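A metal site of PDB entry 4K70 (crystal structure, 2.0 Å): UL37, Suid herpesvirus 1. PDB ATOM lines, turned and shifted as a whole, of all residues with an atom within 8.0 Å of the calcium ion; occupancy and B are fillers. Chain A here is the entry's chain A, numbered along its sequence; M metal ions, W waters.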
ATOM      1  N   VAL A 380       6.468 -22.151   5.033  1.00  0.00           N
ATOM      2  CA  VAL A 380       7.890 -21.898   5.151  1.00  0.00           C
ATOM      3  C   VAL A 380       8.394 -22.380   6.523  1.00  0.00           C
ATOM      4  O   VAL A 380       9.411 -23.076   6.614  1.00  0.00           O
ATOM      5  CB  VAL A 380       8.210 -20.424   4.919  1.00  0.00           C
ATOM      6  CG1 VAL A 380       9.696 -20.145   5.182  1.00  0.00           C
ATOM      7  CG2 VAL A 380       7.817 -20.022   3.483  1.00  0.00           C
ATOM      8  N   VAL A 381       7.674 -22.041   7.574  1.00  0.00           N
ATOM      9  CA  VAL A 381       8.017 -22.536   8.915  1.00  0.00           C
ATOM     10  C   VAL A 381       8.097 -24.072   8.944  1.00  0.00           C
ATOM     11  O   VAL A 381       9.065 -24.636   9.459  1.00  0.00           O
ATOM     12  CB  VAL A 381       6.990 -22.070   9.973  1.00  0.00           C
ATOM     13  CG1 VAL A 381       7.154 -22.835  11.279  1.00  0.00           C
ATOM     14  CG2 VAL A 381       7.118 -20.567  10.183  1.00  0.00           C
ATOM     15  N   HIS A 382       7.089 -24.745   8.398  1.00  0.00           N
ATOM     16  CA  HIS A 382       7.062 -26.223   8.400  1.00  0.00           C
ATOM     17  C   HIS A 382       8.260 -26.823   7.683  1.00  0.00           C
ATOM     18  O   HIS A 382       8.829 -27.837   8.123  1.00  0.00           O
ATOM     19  CB  HIS A 382       5.756 -26.748   7.797  1.00  0.00           C
ATOM     20  CG  HIS A 382       4.611 -26.728   8.754  1.00  0.00           C
ATOM     21  ND1 HIS A 382       4.582 -27.498   9.898  1.00  0.00           N
ATOM     22  CD2 HIS A 382       3.450 -26.022   8.748  1.00  0.00           C
ATOM     23  CE1 HIS A 382       3.452 -27.272  10.557  1.00  0.00           C
ATOM     24  NE2 HIS A 382       2.750 -26.384   9.881  1.00  0.00           N
ATOM     25  N   ARG A 383       8.632 -26.196   6.564  1.00  0.00           N
ATOM     26  CA  ARG A 383       9.822 -26.588   5.826  1.00  0.00           C
ATOM     27  C   ARG A 383      11.101 -26.482   6.641  1.00  0.00           C
ATOM     28  O   ARG A 383      11.963 -27.342   6.565  1.00  0.00           O
ATOM     29  CB  ARG A 383       9.971 -25.703   4.585  1.00  0.00           C
ATOM     30  CG  ARG A 383       9.051 -26.065   3.463  1.00  0.00           C
ATOM     31  CD  ARG A 383       9.692 -25.654   2.167  1.00  0.00           C
ATOM     32  NE  ARG A 383       9.367 -24.311   1.731  1.00  0.00           N
ATOM     33  CZ  ARG A 383      10.211 -23.535   1.045  1.00  0.00           C
ATOM     34  NH1 ARG A 383      11.442 -23.966   0.757  1.00  0.00           N
ATOM     35  NH2 ARG A 383       9.839 -22.325   0.648  1.00  0.00           N
ATOM     36  N   LEU A 384      11.246 -25.383   7.379  1.00  0.00           N
ATOM     37  CA  LEU A 384      12.457 -25.135   8.163  1.00  0.00           C
ATOM     38  C   LEU A 384      12.550 -25.970   9.423  1.00  0.00           C
ATOM     39  O   LEU A 384      13.650 -26.214   9.921  1.00  0.00           O
ATOM     40  CB  LEU A 384      12.542 -23.658   8.578  1.00  0.00           C
ATOM     41  CG  LEU A 384      12.766 -22.630   7.475  1.00  0.00           C
ATOM     42  CD1 LEU A 384      12.346 -21.252   7.935  1.00  0.00           C
ATOM     43  CD2 LEU A 384      14.220 -22.623   7.061  1.00  0.00           C
ATOM     44  N   LEU A 385      11.407 -26.361   9.974  1.00  0.00           N
ATOM     45  CA  LEU A 385      11.384 -26.902  11.325  1.00  0.00           C
ATOM     46  C   LEU A 385      12.241 -28.160  11.509  1.00  0.00           C
ATOM     47  O   LEU A 385      12.896 -28.315  12.536  1.00  0.00           O
ATOM     48  CB  LEU A 385       9.942 -27.158  11.784  1.00  0.00           C
ATOM     49  CG  LEU A 385       9.792 -27.787  13.172  1.00  0.00           C
ATOM     50  CD1 LEU A 385      10.471 -26.949  14.261  1.00  0.00           C
ATOM     51  CD2 LEU A 385       8.332 -28.049  13.508  1.00  0.00           C
ATOM     52  N   ASP A 386      12.251 -29.057  10.521  1.00  0.00           N
ATOM     53  CA  ASP A 386      13.022 -30.296  10.669  1.00  0.00           C
ATOM     54  C   ASP A 386      14.518 -30.034  10.758  1.00  0.00           C
ATOM     55  O   ASP A 386      15.265 -30.853  11.292  1.00  0.00           O
ATOM     56  CB  ASP A 386      12.706 -31.336   9.556  1.00  0.00           C
ATOM     57  CG  ASP A 386      13.308 -30.969   8.205  1.00  0.00           C
ATOM     58  OD1 ASP A 386      12.664 -30.224   7.432  1.00  0.00           O
ATOM     59  OD2 ASP A 386      14.438 -31.437   7.903  1.00  0.00           O
ATOM     60  N   ASP A 387      14.959 -28.883  10.264  1.00  0.00           N
ATOM     61  CA  ASP A 387      16.377 -28.595  10.201  1.00  0.00           C
ATOM     62  C   ASP A 387      16.817 -27.749  11.386  1.00  0.00           C
ATOM     63  O   ASP A 387      18.005 -27.566  11.607  1.00  0.00           O
ATOM     64  CB  ASP A 387      16.685 -27.840   8.930  1.00  0.00           C
ATOM     65  CG  ASP A 387      16.302 -28.616   7.698  1.00  0.00           C
ATOM     66  OD1 ASP A 387      16.989 -29.632   7.418  1.00  0.00           O
ATOM     67  OD2 ASP A 387      15.329 -28.222   7.035  1.00  0.00           O
ATOM     68  N   TYR A 388      15.855 -27.265  12.148  1.00  0.00           N
ATOM     69  CA  TYR A 388      16.124 -26.227  13.141  1.00  0.00           C
ATOM     70  C   TYR A 388      17.130 -26.634  14.213  1.00  0.00           C
ATOM     71  O   TYR A 388      16.948 -27.654  14.885  1.00  0.00           O
ATOM     72  CB  TYR A 388      14.835 -25.765  13.818  1.00  0.00           C
ATOM     73  CG  TYR A 388      15.073 -24.530  14.655  1.00  0.00           C
ATOM     74  CD1 TYR A 388      15.522 -24.617  15.970  1.00  0.00           C
ATOM     75  CD2 TYR A 388      14.893 -23.271  14.100  1.00  0.00           C
ATOM     76  CE1 TYR A 388      15.761 -23.479  16.715  1.00  0.00           C
ATOM     77  CE2 TYR A 388      15.125 -22.130  14.839  1.00  0.00           C
ATOM     78  CZ  TYR A 388      15.563 -22.244  16.153  1.00  0.00           C
ATOM     79  OH  TYR A 388      15.775 -21.102  16.867  1.00  0.00           O
ATOM     80  N   TYR A 394      21.915 -25.717   9.991  1.00  0.00           N
ATOM     81  CA  TYR A 394      20.655 -24.957   9.947  1.00  0.00           C
ATOM     82  C   TYR A 394      20.864 -23.598   9.273  1.00  0.00           C
ATOM     83  O   TYR A 394      19.989 -23.150   8.543  1.00  0.00           O
ATOM     84  CB  TYR A 394      20.007 -24.797  11.321  1.00  0.00           C
ATOM     85  CG  TYR A 394      18.699 -24.033  11.238  1.00  0.00           C
ATOM     86  CD1 TYR A 394      17.659 -24.498  10.449  1.00  0.00           C
ATOM     87  CD2 TYR A 394      18.517 -22.835  11.930  1.00  0.00           C
ATOM     88  CE1 TYR A 394      16.449 -23.810  10.364  1.00  0.00           C
ATOM     89  CE2 TYR A 394      17.322 -22.144  11.846  1.00  0.00           C
ATOM     90  CZ  TYR A 394      16.285 -22.635  11.057  1.00  0.00           C
ATOM     91  OH  TYR A 394      15.093 -21.960  10.962  1.00  0.00           O
ATOM     92  N   ALA A 397      20.566 -24.553   5.727  1.00  0.00           N
ATOM     93  CA  ALA A 397      19.198 -24.937   5.366  1.00  0.00           C
ATOM     94  C   ALA A 397      18.291 -23.707   5.316  1.00  0.00           C
ATOM     95  O   ALA A 397      17.421 -23.600   4.458  1.00  0.00           O
ATOM     96  CB  ALA A 397      18.650 -25.933   6.341  1.00  0.00           C
ATOM     97  N   TYR A 398      18.516 -22.764   6.237  1.00  0.00           N
ATOM     98  CA  TYR A 398      17.722 -21.535   6.296  1.00  0.00           C
ATOM     99  C   TYR A 398      17.983 -20.641   5.077  1.00  0.00           C
ATOM    100  O   TYR A 398      17.060 -20.131   4.457  1.00  0.00           O
ATOM    101  CB  TYR A 398      18.035 -20.755   7.575  1.00  0.00           C
ATOM    102  CG  TYR A 398      17.247 -19.461   7.703  1.00  0.00           C
ATOM    103  CD1 TYR A 398      15.997 -19.446   8.291  1.00  0.00           C
ATOM    104  CD2 TYR A 398      17.751 -18.259   7.225  1.00  0.00           C
ATOM    105  CE1 TYR A 398      15.256 -18.269   8.407  1.00  0.00           C
ATOM    106  CE2 TYR A 398      17.006 -17.058   7.340  1.00  0.00           C
ATOM    107  CZ  TYR A 398      15.776 -17.081   7.936  1.00  0.00           C
ATOM    108  OH  TYR A 398      15.027 -15.909   8.075  1.00  0.00           O
ATOM    109  N   VAL A 401      16.203 -21.937   2.011  1.00  0.00           N
ATOM    110  CA  VAL A 401      14.794 -21.605   2.047  1.00  0.00           C
ATOM    111  C   VAL A 401      14.573 -20.109   1.798  1.00  0.00           C
ATOM    112  O   VAL A 401      13.708 -19.739   1.006  1.00  0.00           O
ATOM    113  CB  VAL A 401      14.156 -22.027   3.395  1.00  0.00           C
ATOM    114  CG1 VAL A 401      12.793 -21.366   3.576  1.00  0.00           C
ATOM    115  CG2 VAL A 401      14.051 -23.559   3.490  1.00  0.00           C
HETATM  116 CA    CA M   1      13.589 -28.882   5.701  1.00  0.00          CA
HETATM  117  O   HOH W   1      14.491 -27.232   4.196  1.00  0.00           O
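The calcium ion is bound by the side-chain carboxylate of Asp 387 (2.3 Å), the side-chain carboxylate of Asp 386 (2.4 Å), the backbone carbonyl oxygen of Arg 383 (2.4 Å) and water W1 (2.4 Å).
The calcium ion has four donor atoms within binding distance.
Of the 13 residues printed, 3 come within 4 Å of the calcium ion.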
